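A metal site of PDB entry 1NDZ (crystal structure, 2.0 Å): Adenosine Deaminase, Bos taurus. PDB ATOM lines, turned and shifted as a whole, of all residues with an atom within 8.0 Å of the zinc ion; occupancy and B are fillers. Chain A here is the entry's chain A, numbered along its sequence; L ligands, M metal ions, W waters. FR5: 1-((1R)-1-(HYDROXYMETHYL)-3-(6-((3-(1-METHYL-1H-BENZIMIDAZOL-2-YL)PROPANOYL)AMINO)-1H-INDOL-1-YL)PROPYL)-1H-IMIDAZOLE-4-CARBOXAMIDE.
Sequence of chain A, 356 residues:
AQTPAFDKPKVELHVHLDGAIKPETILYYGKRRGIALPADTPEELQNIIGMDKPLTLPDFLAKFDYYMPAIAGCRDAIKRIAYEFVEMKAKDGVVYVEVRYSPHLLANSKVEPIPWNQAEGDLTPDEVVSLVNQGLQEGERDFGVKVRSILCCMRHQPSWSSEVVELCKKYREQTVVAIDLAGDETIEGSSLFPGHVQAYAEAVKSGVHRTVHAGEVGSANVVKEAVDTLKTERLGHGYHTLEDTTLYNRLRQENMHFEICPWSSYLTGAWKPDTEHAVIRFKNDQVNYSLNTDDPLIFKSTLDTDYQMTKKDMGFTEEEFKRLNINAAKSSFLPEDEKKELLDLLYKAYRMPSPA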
ATOM      1  N   HIS A  14      -3.638  17.077 -16.016  1.00  0.00           N
ATOM      2  CA  HIS A  14      -2.474  16.091 -16.011  1.00  0.00           C
ATOM      3  C   HIS A  14      -2.992  14.558 -16.204  1.00  0.00           C
ATOM      4  O   HIS A  14      -3.165  13.816 -15.291  1.00  0.00           O
ATOM      5  CB  HIS A  14      -1.507  16.284 -14.788  1.00  0.00           C
ATOM      6  CG  HIS A  14      -0.174  15.553 -14.946  1.00  0.00           C
ATOM      7  ND1 HIS A  14       1.042  16.118 -14.743  1.00  0.00           N
ATOM      8  CD2 HIS A  14       0.055  14.176 -15.228  1.00  0.00           C
ATOM      9  CE1 HIS A  14       2.057  15.149 -14.886  1.00  0.00           C
ATOM     10  NE2 HIS A  14       1.536  13.977 -15.181  1.00  0.00           N
ATOM     11  N   VAL A  15      -3.176  14.198 -17.479  1.00  0.00           N
ATOM     12  CA  VAL A  15      -3.440  12.843 -17.936  1.00  0.00           C
ATOM     13  C   VAL A  15      -2.776  12.614 -19.276  1.00  0.00           C
ATOM     14  O   VAL A  15      -2.610  13.406 -20.192  1.00  0.00           O
ATOM     15  CB  VAL A  15      -4.984  12.545 -17.944  1.00  0.00           C
ATOM     16  CG1 VAL A  15      -5.706  13.503 -18.770  1.00  0.00           C
ATOM     17  CG2 VAL A  15      -5.157  11.193 -18.770  1.00  0.00           C
ATOM     18  N   HIS A  16      -2.188  11.420 -19.326  1.00  0.00           N
ATOM     19  CA  HIS A  16      -1.514  11.105 -20.611  1.00  0.00           C
ATOM     20  C   HIS A  16      -2.334  10.175 -21.647  1.00  0.00           C
ATOM     21  O   HIS A  16      -2.759   9.089 -21.235  1.00  0.00           O
ATOM     22  CB  HIS A  16      -0.151  10.221 -20.398  1.00  0.00           C
ATOM     23  CG  HIS A  16       0.925  10.780 -19.499  1.00  0.00           C
ATOM     24  ND1 HIS A  16       2.037  11.182 -20.085  1.00  0.00           N
ATOM     25  CD2 HIS A  16       0.970  11.101 -18.121  1.00  0.00           C
ATOM     26  CE1 HIS A  16       2.770  11.735 -19.007  1.00  0.00           C
ATOM     27  NE2 HIS A  16       2.184  11.815 -17.717  1.00  0.00           N
ATOM     28  N   ARG A 100      -2.063  14.921 -22.681  1.00  0.00           N
ATOM     29  CA  ARG A 100      -0.694  15.087 -23.141  1.00  0.00           C
ATOM     30  C   ARG A 100      -0.141  13.713 -23.564  1.00  0.00           C
ATOM     31  O   ARG A 100      -0.696  12.665 -23.172  1.00  0.00           O
ATOM     32  CB  ARG A 100       0.219  15.542 -21.968  1.00  0.00           C
ATOM     33  CG  ARG A 100       0.474  14.498 -20.805  1.00  0.00           C
ATOM     34  CD  ARG A 100       1.220  15.121 -19.511  1.00  0.00           C
ATOM     35  NE  ARG A 100       0.554  16.405 -19.163  1.00  0.00           N
ATOM     36  CZ  ARG A 100       1.074  17.185 -18.242  1.00  0.00           C
ATOM     37  NH1 ARG A 100       2.337  16.980 -17.937  1.00  0.00           N
ATOM     38  NH2 ARG A 100       0.388  18.187 -17.574  1.00  0.00           N
ATOM     39  N   CYS A 152       4.826  16.258 -25.250  1.00  0.00           N
ATOM     40  CA  CYS A 152       5.912  15.978 -24.357  1.00  0.00           C
ATOM     41  C   CYS A 152       7.182  15.687 -25.075  1.00  0.00           C
ATOM     42  O   CYS A 152       7.262  14.864 -25.969  1.00  0.00           O
ATOM     43  CB  CYS A 152       5.526  14.635 -23.786  1.00  0.00           C
ATOM     44  SG  CYS A 152       3.990  14.529 -22.719  1.00  0.00           S
ATOM     45  N   ASP A 180       5.543  19.953 -22.706  1.00  0.00           N
ATOM     46  CA  ASP A 180       5.816  19.254 -21.466  1.00  0.00           C
ATOM     47  C   ASP A 180       7.200  18.441 -21.569  1.00  0.00           C
ATOM     48  O   ASP A 180       7.789  18.355 -22.612  1.00  0.00           O
ATOM     49  CB  ASP A 180       4.654  18.267 -20.999  1.00  0.00           C
ATOM     50  CG  ASP A 180       4.901  17.458 -19.701  1.00  0.00           C
ATOM     51  OD1 ASP A 180       4.531  16.281 -19.633  1.00  0.00           O
ATOM     52  OD2 ASP A 180       5.416  18.023 -18.694  1.00  0.00           O
ATOM     53  N   LEU A 181       7.622  18.053 -20.395  1.00  0.00           N
ATOM     54  CA  LEU A 181       8.912  17.214 -20.221  1.00  0.00           C
ATOM     55  C   LEU A 181       8.626  16.057 -19.334  1.00  0.00           C
ATOM     56  O   LEU A 181       8.423  16.138 -18.202  1.00  0.00           O
ATOM     57  CB  LEU A 181      10.166  18.126 -19.895  1.00  0.00           C
ATOM     58  CG  LEU A 181      11.511  17.217 -19.656  1.00  0.00           C
ATOM     59  CD1 LEU A 181      12.029  16.560 -21.039  1.00  0.00           C
ATOM     60  CD2 LEU A 181      12.666  18.312 -19.183  1.00  0.00           C
ATOM     61  N   ALA A 182       8.666  14.923 -20.014  1.00  0.00           N
ATOM     62  CA  ALA A 182       8.299  13.696 -19.328  1.00  0.00           C
ATOM     63  C   ALA A 182       9.397  12.537 -19.621  1.00  0.00           C
ATOM     64  O   ALA A 182      10.402  12.737 -20.268  1.00  0.00           O
ATOM     65  CB  ALA A 182       7.122  13.216 -20.150  1.00  0.00           C
ATOM     66  N   GLY A 183       9.172  11.343 -18.996  1.00  0.00           N
ATOM     67  CA  GLY A 183      10.287  10.353 -18.859  1.00  0.00           C
ATOM     68  C   GLY A 183      10.872  10.153 -17.559  1.00  0.00           C
ATOM     69  O   GLY A 183      10.336  10.480 -16.521  1.00  0.00           O
ATOM     70  N   HIS A 213       7.283  17.695 -15.917  1.00  0.00           N
ATOM     71  CA  HIS A 213       7.275  16.785 -14.828  1.00  0.00           C
ATOM     72  C   HIS A 213       8.578  16.836 -13.946  1.00  0.00           C
ATOM     73  O   HIS A 213       9.683  16.717 -14.407  1.00  0.00           O
ATOM     74  CB  HIS A 213       7.199  15.178 -15.164  1.00  0.00           C
ATOM     75  CG  HIS A 213       5.980  14.668 -15.841  1.00  0.00           C
ATOM     76  ND1 HIS A 213       5.538  15.166 -16.910  1.00  0.00           N
ATOM     77  CD2 HIS A 213       5.193  13.530 -15.531  1.00  0.00           C
ATOM     78  CE1 HIS A 213       4.484  14.411 -17.328  1.00  0.00           C
ATOM     79  NE2 HIS A 213       4.262  13.396 -16.521  1.00  0.00           N
ATOM     80  N   GLU A 216       8.554  14.388  -8.727  1.00  0.00           N
ATOM     81  CA  GLU A 216       7.683  13.183  -8.567  1.00  0.00           C
ATOM     82  C   GLU A 216       8.445  12.049  -7.819  1.00  0.00           C
ATOM     83  O   GLU A 216       8.049  11.698  -6.711  1.00  0.00           O
ATOM     84  CB  GLU A 216       7.054  12.663  -9.878  1.00  0.00           C
ATOM     85  CG  GLU A 216       6.256  11.324  -9.720  1.00  0.00           C
ATOM     86  CD  GLU A 216       5.795  10.789 -11.023  1.00  0.00           C
ATOM     87  OE1 GLU A 216       6.468  11.122 -11.924  1.00  0.00           O
ATOM     88  OE2 GLU A 216       4.901   9.971 -11.166  1.00  0.00           O
ATOM     89  N   GLY A 236       4.466  19.244 -12.980  1.00  0.00           N
ATOM     90  CA  GLY A 236       3.929  17.861 -12.894  1.00  0.00           C
ATOM     91  C   GLY A 236       4.381  17.212 -11.563  1.00  0.00           C
ATOM     92  O   GLY A 236       5.568  16.948 -11.355  1.00  0.00           O
ATOM     93  N   HIS A 237       3.353  17.038 -10.706  1.00  0.00           N
ATOM     94  CA  HIS A 237       3.452  16.404  -9.384  1.00  0.00           C
ATOM     95  C   HIS A 237       4.212  17.390  -8.424  1.00  0.00           C
ATOM     96  O   HIS A 237       3.706  18.110  -7.594  1.00  0.00           O
ATOM     97  CB  HIS A 237       4.311  15.156  -9.432  1.00  0.00           C
ATOM     98  CG  HIS A 237       3.777  14.044 -10.317  1.00  0.00           C
ATOM     99  ND1 HIS A 237       2.770  13.265  -9.912  1.00  0.00           N
ATOM    100  CD2 HIS A 237       4.110  13.692 -11.627  1.00  0.00           C
ATOM    101  CE1 HIS A 237       2.382  12.437 -10.904  1.00  0.00           C
ATOM    102  NE2 HIS A 237       3.243  12.667 -11.985  1.00  0.00           N
ATOM    103  N   GLU A 259       0.328  20.185 -10.392  1.00  0.00           N
ATOM    104  CA  GLU A 259      -0.509  19.108 -10.947  1.00  0.00           C
ATOM    105  C   GLU A 259      -0.419  17.755 -10.143  1.00  0.00           C
ATOM    106  O   GLU A 259       0.435  16.940 -10.408  1.00  0.00           O
ATOM    107  CB  GLU A 259      -0.042  18.866 -12.363  1.00  0.00           C
ATOM    108  CG  GLU A 259       0.117  20.186 -13.202  1.00  0.00           C
ATOM    109  CD  GLU A 259       0.647  19.937 -14.593  1.00  0.00           C
ATOM    110  OE1 GLU A 259       1.070  18.839 -14.796  1.00  0.00           O
ATOM    111  OE2 GLU A 259       0.587  20.881 -15.431  1.00  0.00           O
ATOM    112  N   CYS A 261      -1.282  14.053  -8.543  1.00  0.00           N
ATOM    113  CA  CYS A 261      -1.913  12.867  -9.006  1.00  0.00           C
ATOM    114  C   CYS A 261      -1.844  11.808  -7.865  1.00  0.00           C
ATOM    115  O   CYS A 261      -0.887  11.071  -7.740  1.00  0.00           O
ATOM    116  CB  CYS A 261      -1.237  12.258 -10.252  1.00  0.00           C
ATOM    117  SG  CYS A 261      -0.853  13.368 -11.608  1.00  0.00           S
ATOM    118  N   SER A 264      -2.026   7.693  -8.510  1.00  0.00           N
ATOM    119  CA  SER A 264      -0.643   7.722  -9.097  1.00  0.00           C
ATOM    120  C   SER A 264       0.590   7.685  -8.197  1.00  0.00           C
ATOM    121  O   SER A 264       1.425   6.760  -8.238  1.00  0.00           O
ATOM    122  CB  SER A 264      -0.556   8.604 -10.300  1.00  0.00           C
ATOM    123  OG  SER A 264       0.773   8.613 -10.806  1.00  0.00           O
ATOM    124  N   THR A 293      -5.473  12.240 -12.773  1.00  0.00           N
ATOM    125  CA  THR A 293      -5.397  10.718 -12.809  1.00  0.00           C
ATOM    126  C   THR A 293      -4.105  10.173 -13.392  1.00  0.00           C
ATOM    127  O   THR A 293      -3.816   9.112 -12.898  1.00  0.00           O
ATOM    128  CB  THR A 293      -6.468  10.214 -13.822  1.00  0.00           C
ATOM    129  OG1 THR A 293      -6.480  10.437 -15.288  1.00  0.00           O
ATOM    130  CG2 THR A 293      -7.881  10.103 -13.302  1.00  0.00           C
ATOM    131  N   ASP A 294      -3.398  10.947 -14.357  1.00  0.00           N
ATOM    132  CA  ASP A 294      -2.140  10.541 -15.023  1.00  0.00           C
ATOM    133  C   ASP A 294      -2.233   9.432 -16.032  1.00  0.00           C
ATOM    134  O   ASP A 294      -2.035   9.662 -17.224  1.00  0.00           O
ATOM    135  CB  ASP A 294      -1.103  10.113 -13.851  1.00  0.00           C
ATOM    136  CG  ASP A 294       0.362  10.411 -14.179  1.00  0.00           C
ATOM    137  OD1 ASP A 294       1.173  10.032 -13.306  1.00  0.00           O
ATOM    138  OD2 ASP A 294       0.654  11.031 -15.226  1.00  0.00           O
ATOM    139  N   ASP A 295      -2.555   8.149 -15.509  1.00  0.00           N
ATOM    140  CA  ASP A 295      -2.561   6.998 -16.497  1.00  0.00           C
ATOM    141  C   ASP A 295      -3.645   5.980 -15.878  1.00  0.00           C
ATOM    142  O   ASP A 295      -3.327   4.974 -15.267  1.00  0.00           O
ATOM    143  CB  ASP A 295      -1.234   6.164 -16.500  1.00  0.00           C
ATOM    144  CG  ASP A 295      -0.062   7.019 -16.940  1.00  0.00           C
ATOM    145  OD1 ASP A 295       0.338   6.911 -18.077  1.00  0.00           O
ATOM    146  OD2 ASP A 295       0.326   7.883 -16.206  1.00  0.00           O
ATOM    147  N   PHE A 299      -3.362   2.568 -13.838  1.00  0.00           N
ATOM    148  CA  PHE A 299      -3.642   2.514 -12.423  1.00  0.00           C
ATOM    149  C   PHE A 299      -5.054   2.006 -12.128  1.00  0.00           C
ATOM    150  O   PHE A 299      -5.614   2.255 -11.042  1.00  0.00           O
ATOM    151  CB  PHE A 299      -3.407   3.944 -11.861  1.00  0.00           C
ATOM    152  CG  PHE A 299      -2.041   4.570 -12.293  1.00  0.00           C
ATOM    153  CD1 PHE A 299      -0.861   3.690 -12.246  1.00  0.00           C
ATOM    154  CD2 PHE A 299      -1.841   5.889 -12.773  1.00  0.00           C
ATOM    155  CE1 PHE A 299       0.440   4.178 -12.350  1.00  0.00           C
ATOM    156  CE2 PHE A 299      -0.542   6.355 -12.980  1.00  0.00           C
ATOM    157  CZ  PHE A 299       0.590   5.548 -12.689  1.00  0.00           C
HETATM  158  C1  FR5 L   1       4.601   8.840 -19.427  1.00  0.00           C
HETATM  159  N2  FR5 L   1       3.880   8.448 -20.537  1.00  0.00           N
HETATM  160  C3  FR5 L   1       2.681   7.992 -20.061  1.00  0.00           C
HETATM  161  N4  FR5 L   1       2.639   7.973 -18.798  1.00  0.00           N
HETATM  162  C5  FR5 L   1       3.916   8.454 -18.384  1.00  0.00           C
HETATM  163  C8  FR5 L   1       4.369   8.558 -16.999  1.00  0.00           C
HETATM  164  O9  FR5 L   1       5.582   8.750 -16.695  1.00  0.00           O
HETATM  165  N10 FR5 L   1       3.416   8.339 -16.114  1.00  0.00           N
HETATM  166  C13 FR5 L   1       4.408   8.379 -21.932  1.00  0.00           C
HETATM  167  C14 FR5 L   1       4.224   9.689 -22.829  1.00  0.00           C
HETATM  168  O15 FR5 L   1       2.980  10.401 -22.846  1.00  0.00           O
HETATM  169  C18 FR5 L   1       5.905   8.079 -21.982  1.00  0.00           C
HETATM  170  C19 FR5 L   1       6.284   6.710 -21.275  1.00  0.00           C
HETATM  171  N22 FR5 L   1       7.828   6.571 -21.071  1.00  0.00           N
HETATM  172  C27 FR5 L   1       8.701   6.273 -22.053  1.00  0.00           C
HETATM  173  C28 FR5 L   1       9.911   6.168 -21.527  1.00  0.00           C
HETATM  174  C29 FR5 L   1       9.721   6.391 -20.098  1.00  0.00           C
HETATM  175  C30 FR5 L   1       8.403   6.728 -19.886  1.00  0.00           C
HETATM  176  C31 FR5 L   1      10.600   6.571 -19.101  1.00  0.00           C
HETATM  177  C32 FR5 L   1      10.161   6.905 -17.917  1.00  0.00           C
HETATM  178  C33 FR5 L   1       8.841   7.166 -17.713  1.00  0.00           C
HETATM  179  C34 FR5 L   1       7.949   7.014 -18.704  1.00  0.00           C
HETATM  180  N1  FR5 L   1       8.304   7.438 -16.581  1.00  0.00           N
HETATM  181  C2  FR5 L   1       8.851   7.599 -15.474  1.00  0.00           C
HETATM  182  O1  FR5 L   1       9.996   7.294 -15.204  1.00  0.00           O
HETATM  183  C4  FR5 L   1       7.985   8.301 -14.418  1.00  0.00           C
HETATM  184  C6  FR5 L   1       8.243   7.963 -12.934  1.00  0.00           C
HETATM  185  C9  FR5 L   1       5.209   2.728 -12.183  1.00  0.00           C
HETATM  186  C15 FR5 L   1       5.247   3.985 -12.812  1.00  0.00           C
HETATM  187  C10 FR5 L   1       6.321   4.841 -12.710  1.00  0.00           C
HETATM  188  C16 FR5 L   1       7.339   4.618 -11.753  1.00  0.00           C
HETATM  189  C11 FR5 L   1       7.357   3.391 -11.132  1.00  0.00           C
HETATM  190  C17 FR5 L   1       6.251   2.484 -11.302  1.00  0.00           C
HETATM  191  N11 FR5 L   1       6.567   6.074 -13.250  1.00  0.00           N
HETATM  192  C12 FR5 L   1       7.695   6.550 -12.695  1.00  0.00           C
HETATM  193  N13 FR5 L   1       8.242   5.693 -11.840  1.00  0.00           N
HETATM  194  C7  FR5 L   1       9.486   5.836 -11.096  1.00  0.00           C
HETATM  195 ZN    ZN M   1       2.438  12.374 -15.908  1.00  0.00          ZN
HETATM  196  O   HOH W   1       3.159  11.469 -14.375  1.00  0.00           O
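The side-chain carboxylate (OE1) of Glu 259 is in hydrogen-bond range of a ring nitrogen (ND1) of His 14, 2.7 Å away.
A ring nitrogen (ND1) of His 213 sits close to the side-chain carboxylate of Asp 180 (3.1 Å).
The backbone carbonyl oxygen of Leu 181 sits at hydrogen-bond distance from the backbone NH of His 213 (3.0 Å).
OD1 of Asp 294 sits at hydrogen-bond distance from OG of Ser 264, at 2.9 Å.
A ring nitrogen (ND1) of His 16 lies within hydrogen-bond range of an oxygen (O15) of the ligand (3.0 Å).
The side-chain carboxylate of Asp 295 sits at hydrogen-bond distance from a nitrogen (N4) of the ligand (2.6 Å).
Water W1 bridges the side-chain carboxylate (OD1) of Asp 294 (2.7 Å) and a ring nitrogen (NE2) of His 237 (2.7 Å).
Four residues have an atom within 4 Å of the zinc ion: His 14, His 16, His 213 and Asp 294.
The zinc ion is bound by NE2 of His 16, water W1, NE2 of His 14, NE2 of His 213 and OD2 of Asp 294.
The zinc ion has five donor atoms within binding distance.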
